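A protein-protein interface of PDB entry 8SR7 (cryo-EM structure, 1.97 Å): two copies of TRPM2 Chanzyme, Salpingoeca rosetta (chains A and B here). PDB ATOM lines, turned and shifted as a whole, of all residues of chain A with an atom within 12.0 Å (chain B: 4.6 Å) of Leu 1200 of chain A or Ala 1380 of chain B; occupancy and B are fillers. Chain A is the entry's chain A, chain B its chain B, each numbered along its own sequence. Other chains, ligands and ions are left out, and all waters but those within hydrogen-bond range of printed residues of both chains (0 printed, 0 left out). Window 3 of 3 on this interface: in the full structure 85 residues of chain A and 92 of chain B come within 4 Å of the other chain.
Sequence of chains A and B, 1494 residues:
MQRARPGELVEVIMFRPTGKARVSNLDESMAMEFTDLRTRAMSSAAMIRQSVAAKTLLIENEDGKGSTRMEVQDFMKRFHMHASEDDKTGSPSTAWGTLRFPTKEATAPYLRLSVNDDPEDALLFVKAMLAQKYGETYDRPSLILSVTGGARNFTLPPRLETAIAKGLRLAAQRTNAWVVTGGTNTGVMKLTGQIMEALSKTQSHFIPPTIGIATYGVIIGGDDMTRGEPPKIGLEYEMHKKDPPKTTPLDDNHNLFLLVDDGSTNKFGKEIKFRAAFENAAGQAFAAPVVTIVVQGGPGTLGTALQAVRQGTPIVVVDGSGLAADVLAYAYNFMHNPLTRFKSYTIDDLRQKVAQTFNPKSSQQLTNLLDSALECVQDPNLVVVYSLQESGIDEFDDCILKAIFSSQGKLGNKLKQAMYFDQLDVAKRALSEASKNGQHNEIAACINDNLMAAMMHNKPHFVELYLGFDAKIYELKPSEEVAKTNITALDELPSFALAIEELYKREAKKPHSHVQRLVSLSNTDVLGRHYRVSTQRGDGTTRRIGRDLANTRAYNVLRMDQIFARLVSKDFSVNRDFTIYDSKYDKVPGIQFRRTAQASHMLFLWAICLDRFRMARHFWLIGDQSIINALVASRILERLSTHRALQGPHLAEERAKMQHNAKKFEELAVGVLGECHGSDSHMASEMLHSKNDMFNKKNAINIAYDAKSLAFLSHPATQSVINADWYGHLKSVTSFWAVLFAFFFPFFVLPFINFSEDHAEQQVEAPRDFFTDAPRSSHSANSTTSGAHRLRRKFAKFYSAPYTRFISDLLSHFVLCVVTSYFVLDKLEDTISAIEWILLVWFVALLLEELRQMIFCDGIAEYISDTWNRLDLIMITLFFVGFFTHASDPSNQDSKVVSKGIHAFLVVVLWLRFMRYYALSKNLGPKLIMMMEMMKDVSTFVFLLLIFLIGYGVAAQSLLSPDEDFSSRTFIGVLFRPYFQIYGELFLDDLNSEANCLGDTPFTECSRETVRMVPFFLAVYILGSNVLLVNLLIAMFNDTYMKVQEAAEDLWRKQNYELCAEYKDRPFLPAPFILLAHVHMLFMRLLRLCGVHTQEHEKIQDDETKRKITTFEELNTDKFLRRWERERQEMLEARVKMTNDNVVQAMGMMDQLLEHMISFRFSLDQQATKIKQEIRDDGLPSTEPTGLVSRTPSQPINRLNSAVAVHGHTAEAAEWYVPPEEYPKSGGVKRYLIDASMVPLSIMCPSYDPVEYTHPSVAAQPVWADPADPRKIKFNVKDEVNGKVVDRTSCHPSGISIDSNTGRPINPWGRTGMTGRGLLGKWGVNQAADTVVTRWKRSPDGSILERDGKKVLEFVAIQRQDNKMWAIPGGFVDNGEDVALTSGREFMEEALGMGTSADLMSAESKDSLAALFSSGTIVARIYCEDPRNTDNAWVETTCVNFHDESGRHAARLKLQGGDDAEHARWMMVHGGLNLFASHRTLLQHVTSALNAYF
The backbone carbonyl oxygen of Gly 1416 of chain B sits at hydrogen-bond distance from the backbone NH of Leu 1200 of chain A (2.7 Å). The side-chain hydroxyl (OG) of Ser 1202 of chain A is in hydrogen-bond range of the backbone carbonyl oxygen (O) of Ala 1380 of chain B (3.0 Å). O of Phe 1413 of chain B sits at hydrogen-bond distance from N of Ser 1202 of chain A (3.1 Å).
Ile 1197 of chain A touches none of the printed residues of chain B. Of the printed residues of chain B, Asn 1198 of chain A touches Ile 1418 (3.7 Å). Leu 1200 of chain A touches just these residues of chain B: Ala 1380 (3.8 Å), Ser 1414 (3.9 Å), Gly 1416 (2.7 Å) and Val 1440 (3.8 Å). Printed residues of chain B within 4 Å of Asn 1201 of chain A: Ala 1380 (3.7 Å) and Ser 1414 (3.7 Å). Of the printed residues of chain B, Val 1206 of chain A touches Phe 1413 (3.7 Å). Thr 1210 of chain A touches none of the printed residues of chain B. Asp 1378 of chain B touches none of the printed residues of chain A. No residue of chain A comes within 4 Å of Val 1379 of chain B. Ala 1380 of chain B touches just these residues of chain A: Leu 1200, Asn 1201 and Ser 1202. Leu 1381 of chain B touches one residue of chain A. No residue of chain A comes within 4 Å of Thr 1382 of chain B. No residue of chain A comes within 4 Å of Ser 1383 of chain B. Gly 1384 of chain B touches just one residue of chain A: Ala 1205 (3.97 Å). Ser 1414 of chain B touches just these residues of chain A: Leu 1200 and Asn 1201. Ser 1415 of chain B touches just one residue of chain A: Arg 1199. Gly 1416 of chain B touches just these residues of chain A: Arg 1199 and Leu 1200. Val 1440 of chain B touches one residue of chain A. The nearest residue of chain A that does not touch Ala 1380 of chain B is Ala 1205 of chain A (4.4 Å). The nearest printed residue of chain B that does not touch Ser 1202 of chain A is Ser 1383 of chain B (4.5 Å).
Of the 13 printed residues of chain B, 9 touch a printed residue of chain A. Printed residues of chain B that touch a printed residue of chain A: Ala 1380, Leu 1381, Gly 1384, Phe 1413, Ser 1414, Ser 1415, Gly 1416, Ile 1418 and Val 1440. Among the printed residues, 15 pairs touch across the chains. Among the printed residues, no Asp or Glu carboxylate lies within 4 Å of a Lys or Arg side-chain nitrogen of the other chain.
No position is printed for both chains.
OD1 of Asn 1201 of chain A lies within hydrogen-bond range of N of Ala 1203 of chain A (3.3 Å).
Among the printed residues, merely in contact across the chains: Arg 1199 of chain A with Gly 1416 of chain B, Ala 1205 of chain A with Leu 1381 of chain B, Asn 1201 of chain A with Ser 1414 of chain B, Asn 1198 of chain A with Ile 1418 of chain B, Asn 1201 of chain A with Ala 1380 of chain B, Val 1206 of chain A with Phe 1413 of chain B, Leu 1200 of chain A with Val 1440 of chain B, Leu 1200 of chain A with Ala 1380 of chain B, Ala 1203 of chain A with Phe 1413 of chain B, Arg 1199 of chain A with Ser 1415 of chain B, Leu 1200 of chain A with Ser 1414 of chain B and Ala 1205 of chain A with Gly 1384 of chain B.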
ATOM      1  N   ILE A1197     -18.297  20.326  26.035  1.00  0.00           N
ATOM      2  CA  ILE A1197     -17.458  20.743  27.150  1.00  0.00           C
ATOM      3  C   ILE A1197     -16.155  19.952  27.156  1.00  0.00           C
ATOM      4  O   ILE A1197     -15.097  20.485  27.488  1.00  0.00           O
ATOM      5  CB  ILE A1197     -18.195  20.588  28.490  1.00  0.00           C
ATOM      6  N   ASN A1198     -16.238  18.673  26.786  1.00  0.00           N
ATOM      7  CA  ASN A1198     -15.075  17.783  26.713  1.00  0.00           C
ATOM      8  C   ASN A1198     -14.381  17.861  25.347  1.00  0.00           C
ATOM      9  O   ASN A1198     -14.327  16.894  24.589  1.00  0.00           O
ATOM     10  CB  ASN A1198     -15.492  16.353  27.034  1.00  0.00           C
ATOM     11  N   ARG A1199     -13.842  19.040  25.038  1.00  0.00           N
ATOM     12  CA  ARG A1199     -13.148  19.289  23.783  1.00  0.00           C
ATOM     13  C   ARG A1199     -11.997  20.241  24.050  1.00  0.00           C
ATOM     14  O   ARG A1199     -12.205  21.327  24.599  1.00  0.00           O
ATOM     15  CB  ARG A1199     -14.093  19.882  22.734  1.00  0.00           C
ATOM     16  CG  ARG A1199     -13.436  20.202  21.401  1.00  0.00           C
ATOM     17  CD  ARG A1199     -12.955  18.959  20.677  1.00  0.00           C
ATOM     18  NE  ARG A1199     -14.062  18.096  20.284  1.00  0.00           N
ATOM     19  CZ  ARG A1199     -13.922  16.854  19.843  1.00  0.00           C
ATOM     20  NH1 ARG A1199     -12.729  16.304  19.695  1.00  0.00           N
ATOM     21  NH2 ARG A1199     -15.007  16.148  19.538  1.00  0.00           N
ATOM     22  N   LEU A1200     -10.788  19.838  23.669  1.00  0.00           N
ATOM     23  CA  LEU A1200      -9.596  20.603  23.990  1.00  0.00           C
ATOM     24  C   LEU A1200      -8.749  20.737  22.730  1.00  0.00           C
ATOM     25  O   LEU A1200      -8.589  19.771  21.979  1.00  0.00           O
ATOM     26  CB  LEU A1200      -8.813  19.929  25.130  1.00  0.00           C
ATOM     27  CG  LEU A1200      -7.597  20.664  25.683  1.00  0.00           C
ATOM     28  CD1 LEU A1200      -8.093  21.965  26.288  1.00  0.00           C
ATOM     29  CD2 LEU A1200      -6.878  19.853  26.712  1.00  0.00           C
ATOM     30  N   ASN A1201      -8.196  21.931  22.505  1.00  0.00           N
ATOM     31  CA  ASN A1201      -7.358  22.218  21.345  1.00  0.00           C
ATOM     32  C   ASN A1201      -5.955  22.479  21.887  1.00  0.00           C
ATOM     33  O   ASN A1201      -5.718  23.483  22.566  1.00  0.00           O
ATOM     34  CB  ASN A1201      -7.920  23.419  20.577  1.00  0.00           C
ATOM     35  CG  ASN A1201      -7.407  23.530  19.134  1.00  0.00           C
ATOM     36  OD1 ASN A1201      -6.251  23.259  18.821  1.00  0.00           O
ATOM     37  ND2 ASN A1201      -8.301  23.940  18.245  1.00  0.00           N
ATOM     38  N   SER A1202      -5.030  21.569  21.576  1.00  0.00           N
ATOM     39  CA  SER A1202      -3.648  21.620  22.038  1.00  0.00           C
ATOM     40  C   SER A1202      -2.660  21.999  20.942  1.00  0.00           C
ATOM     41  O   SER A1202      -1.471  21.692  21.068  1.00  0.00           O
ATOM     42  CB  SER A1202      -3.238  20.289  22.656  1.00  0.00           C
ATOM     43  OG  SER A1202      -3.878  20.084  23.902  1.00  0.00           O
ATOM     44  N   ALA A1203      -3.136  22.604  19.843  1.00  0.00           N
ATOM     45  CA  ALA A1203      -2.269  23.041  18.746  1.00  0.00           C
ATOM     46  C   ALA A1203      -1.348  24.208  19.110  1.00  0.00           C
ATOM     47  O   ALA A1203      -0.369  24.431  18.389  1.00  0.00           O
ATOM     48  CB  ALA A1203      -3.106  23.423  17.527  1.00  0.00           C
ATOM     49  N   VAL A1204      -1.693  24.999  20.144  1.00  0.00           N
ATOM     50  CA  VAL A1204      -0.892  26.123  20.645  1.00  0.00           C
ATOM     51  C   VAL A1204       0.482  25.666  21.186  1.00  0.00           C
ATOM     52  O   VAL A1204       1.473  26.402  21.081  1.00  0.00           O
ATOM     53  CB  VAL A1204      -1.762  26.909  21.674  1.00  0.00           C
ATOM     54  CG1 VAL A1204      -2.279  26.029  22.828  1.00  0.00           C
ATOM     55  CG2 VAL A1204      -1.131  28.228  22.174  1.00  0.00           C
ATOM     56  N   ALA A1205       0.573  24.431  21.719  1.00  0.00           N
ATOM     57  CA  ALA A1205       1.816  23.819  22.192  1.00  0.00           C
ATOM     58  C   ALA A1205       2.823  23.523  21.081  1.00  0.00           C
ATOM     59  O   ALA A1205       4.024  23.445  21.359  1.00  0.00           O
ATOM     60  CB  ALA A1205       1.506  22.528  22.948  1.00  0.00           C
ATOM     61  N   VAL A1206       2.365  23.348  19.842  1.00  0.00           N
ATOM     62  CA  VAL A1206       3.230  22.956  18.737  1.00  0.00           C
ATOM     63  C   VAL A1206       3.700  24.231  18.041  1.00  0.00           C
ATOM     64  O   VAL A1206       4.906  24.448  17.879  1.00  0.00           O
ATOM     65  CB  VAL A1206       2.507  21.979  17.784  1.00  0.00           C
ATOM     66  CG1 VAL A1206       3.168  21.891  16.391  1.00  0.00           C
ATOM     67  CG2 VAL A1206       2.390  20.619  18.424  1.00  0.00           C
ATOM     68  N   HIS A1207       2.757  25.082  17.627  1.00  0.00           N
ATOM     69  CA  HIS A1207       3.114  26.268  16.856  1.00  0.00           C
ATOM     70  C   HIS A1207       3.584  27.403  17.757  1.00  0.00           C
ATOM     71  O   HIS A1207       4.719  27.877  17.636  1.00  0.00           O
ATOM     72  CB  HIS A1207       1.918  26.712  16.010  1.00  0.00           C
ATOM     73  CG  HIS A1207       1.678  25.854  14.808  1.00  0.00           C
ATOM     74  ND1 HIS A1207       2.704  25.352  14.036  1.00  0.00           N
ATOM     75  CD2 HIS A1207       0.531  25.398  14.252  1.00  0.00           C
ATOM     76  CE1 HIS A1207       2.198  24.631  13.051  1.00  0.00           C
ATOM     77  NE2 HIS A1207       0.882  24.643  13.160  1.00  0.00           N
ATOM     78  N   GLY A1208       2.727  27.851  18.668  1.00  0.00           N
ATOM     79  CA  GLY A1208       3.090  28.942  19.550  1.00  0.00           C
ATOM     80  C   GLY A1208       2.324  30.216  19.269  1.00  0.00           C
ATOM     81  O   GLY A1208       2.409  30.734  18.147  1.00  0.00           O
ATOM     82  N   HIS A1209       1.455  30.607  20.227  1.00  0.00           N
ATOM     83  CA  HIS A1209       0.674  31.852  20.366  1.00  0.00           C
ATOM     84  C   HIS A1209      -0.505  32.064  19.408  1.00  0.00           C
ATOM     85  O   HIS A1209      -1.341  32.929  19.700  1.00  0.00           O
ATOM     86  CB  HIS A1209       1.575  33.104  20.332  1.00  0.00           C
ATOM     87  N   THR A1210      -0.635  31.213  18.367  1.00  0.00           N
ATOM     88  CA  THR A1210      -1.655  31.128  17.308  1.00  0.00           C
ATOM     89  C   THR A1210      -2.027  32.471  16.658  1.00  0.00           C
ATOM     90  O   THR A1210      -1.109  33.133  16.153  1.00  0.00           O
ATOM     91  CB  THR A1210      -2.893  30.419  17.879  1.00  0.00           C
ATOM     92  N   ASP B1378      -2.329  26.423  31.223  1.00  0.00           N
ATOM     93  CA  ASP B1378      -3.496  25.560  31.260  1.00  0.00           C
ATOM     94  C   ASP B1378      -3.114  24.139  30.842  1.00  0.00           C
ATOM     95  O   ASP B1378      -1.951  23.851  30.562  1.00  0.00           O
ATOM     96  CB  ASP B1378      -4.629  26.154  30.407  1.00  0.00           C
ATOM     97  CG  ASP B1378      -4.234  26.419  28.944  1.00  0.00           C
ATOM     98  OD1 ASP B1378      -3.042  26.352  28.564  1.00  0.00           O
ATOM     99  OD2 ASP B1378      -5.155  26.704  28.150  1.00  0.00           O
ATOM    100  N   VAL B1379      -4.113  23.245  30.844  1.00  0.00           N
ATOM    101  CA  VAL B1379      -3.950  21.824  30.517  1.00  0.00           C
ATOM    102  C   VAL B1379      -3.616  21.618  29.029  1.00  0.00           C
ATOM    103  O   VAL B1379      -2.895  20.660  28.679  1.00  0.00           O
ATOM    104  CB  VAL B1379      -5.248  21.111  30.977  1.00  0.00           C
ATOM    105  CG1 VAL B1379      -5.238  19.586  30.815  1.00  0.00           C
ATOM    106  CG2 VAL B1379      -5.564  21.473  32.424  1.00  0.00           C
ATOM    107  N   ALA B1380      -4.125  22.531  28.165  1.00  0.00           N
ATOM    108  CA  ALA B1380      -3.952  22.552  26.701  1.00  0.00           C
ATOM    109  C   ALA B1380      -2.487  22.623  26.275  1.00  0.00           C
ATOM    110  O   ALA B1380      -2.045  21.861  25.409  1.00  0.00           O
ATOM    111  CB  ALA B1380      -4.713  23.736  26.110  1.00  0.00           C
ATOM    112  N   LEU B1381      -1.758  23.601  26.822  1.00  0.00           N
ATOM    113  CA  LEU B1381      -0.331  23.759  26.564  1.00  0.00           C
ATOM    114  C   LEU B1381       0.474  22.617  27.182  1.00  0.00           C
ATOM    115  O   LEU B1381       1.424  22.123  26.556  1.00  0.00           O
ATOM    116  CB  LEU B1381       0.135  25.112  27.104  1.00  0.00           C
ATOM    117  CG  LEU B1381       1.604  25.530  27.056  1.00  0.00           C
ATOM    118  CD1 LEU B1381       2.168  25.447  25.653  1.00  0.00           C
ATOM    119  CD2 LEU B1381       1.745  26.941  27.594  1.00  0.00           C
ATOM    120  N   THR B1382       0.091  22.216  28.416  1.00  0.00           N
ATOM    121  CA  THR B1382       0.828  21.261  29.257  1.00  0.00           C
ATOM    122  C   THR B1382       0.870  19.854  28.670  1.00  0.00           C
ATOM    123  O   THR B1382       1.954  19.260  28.630  1.00  0.00           O
ATOM    124  CB  THR B1382       0.196  21.222  30.652  1.00  0.00           C
ATOM    125  OG1 THR B1382       0.068  22.559  31.146  1.00  0.00           O
ATOM    126  CG2 THR B1382       1.033  20.427  31.643  1.00  0.00           C
ATOM    127  N   SER B1383      -0.295  19.359  28.183  1.00  0.00           N
ATOM    128  CA  SER B1383      -0.480  18.012  27.609  1.00  0.00           C
ATOM    129  C   SER B1383       0.380  17.808  26.368  1.00  0.00           C
ATOM    130  O   SER B1383       1.126  16.812  26.264  1.00  0.00           O
ATOM    131  CB  SER B1383      -1.952  17.795  27.265  1.00  0.00           C
ATOM    132  OG  SER B1383      -2.749  17.825  28.429  1.00  0.00           O
ATOM    133  N   GLY B1384       0.271  18.777  25.444  1.00  0.00           N
ATOM    134  CA  GLY B1384       1.039  18.795  24.212  1.00  0.00           C
ATOM    135  C   GLY B1384       2.532  18.939  24.439  1.00  0.00           C
ATOM    136  O   GLY B1384       3.307  18.182  23.851  1.00  0.00           O
ATOM    137  N   PHE B1413      -3.251  17.197  17.117  1.00  0.00           N
ATOM    138  CA  PHE B1413      -3.467  17.795  18.432  1.00  0.00           C
ATOM    139  C   PHE B1413      -4.662  18.739  18.483  1.00  0.00           C
ATOM    140  O   PHE B1413      -4.983  19.242  19.563  1.00  0.00           O
ATOM    141  CB  PHE B1413      -2.213  18.567  18.877  1.00  0.00           C
ATOM    142  CG  PHE B1413      -1.114  17.727  19.521  1.00  0.00           C
ATOM    143  CD1 PHE B1413      -1.093  16.313  19.466  1.00  0.00           C
ATOM    144  CD2 PHE B1413      -0.048  18.398  20.138  1.00  0.00           C
ATOM    145  CE1 PHE B1413      -0.051  15.589  20.055  1.00  0.00           C
ATOM    146  CE2 PHE B1413       1.009  17.689  20.716  1.00  0.00           C
ATOM    147  CZ  PHE B1413       0.995  16.287  20.679  1.00  0.00           C
ATOM    148  N   SER B1414      -5.319  19.000  17.356  1.00  0.00           N
ATOM    149  CA  SER B1414      -6.450  19.920  17.335  1.00  0.00           C
ATOM    150  C   SER B1414      -7.764  19.285  17.768  1.00  0.00           C
ATOM    151  O   SER B1414      -8.720  20.018  18.043  1.00  0.00           O
ATOM    152  CB  SER B1414      -6.617  20.514  15.935  1.00  0.00           C
ATOM    153  OG  SER B1414      -6.698  19.490  14.960  1.00  0.00           O
ATOM    154  N   SER B1415      -7.845  17.957  17.842  1.00  0.00           N
ATOM    155  CA  SER B1415      -9.080  17.266  18.212  1.00  0.00           C
ATOM    156  C   SER B1415      -8.797  16.346  19.394  1.00  0.00           C
ATOM    157  O   SER B1415      -8.475  15.169  19.215  1.00  0.00           O
ATOM    158  CB  SER B1415      -9.641  16.493  17.025  1.00  0.00           C
ATOM    159  OG  SER B1415      -8.651  15.652  16.458  1.00  0.00           O
ATOM    160  N   GLY B1416      -8.915  16.886  20.596  1.00  0.00           N
ATOM    161  CA  GLY B1416      -8.713  16.121  21.817  1.00  0.00           C
ATOM    162  C   GLY B1416      -9.923  16.202  22.724  1.00  0.00           C
ATOM    163  O   GLY B1416     -10.558  17.251  22.827  1.00  0.00           O
ATOM    164  N   ILE B1418     -11.292  15.438  26.667  1.00  0.00           N
ATOM    165  CA  ILE B1418     -10.952  15.176  28.061  1.00  0.00           C
ATOM    166  C   ILE B1418     -11.815  14.001  28.515  1.00  0.00           C
ATOM    167  O   ILE B1418     -13.042  14.110  28.596  1.00  0.00           O
ATOM    168  CB  ILE B1418     -11.164  16.415  28.938  1.00  0.00           C
ATOM    169  CG1 ILE B1418     -10.146  17.494  28.553  1.00  0.00           C
ATOM    170  CG2 ILE B1418     -10.983  16.065  30.422  1.00  0.00           C
ATOM    171  CD1 ILE B1418     -10.258  18.802  29.330  1.00  0.00           C
ATOM    172  N   VAL B1440      -6.159  13.637  28.586  1.00  0.00           N
ATOM    173  CA  VAL B1440      -6.551  14.118  27.264  1.00  0.00           C
ATOM    174  C   VAL B1440      -6.197  13.046  26.247  1.00  0.00           C
ATOM    175  O   VAL B1440      -5.039  12.616  26.167  1.00  0.00           O
ATOM    176  CB  VAL B1440      -5.857  15.441  26.888  1.00  0.00           C
ATOM    177  CG1 VAL B1440      -6.529  16.055  25.677  1.00  0.00           C
ATOM    178  CG2 VAL B1440      -5.832  16.434  28.041  1.00  0.00           C
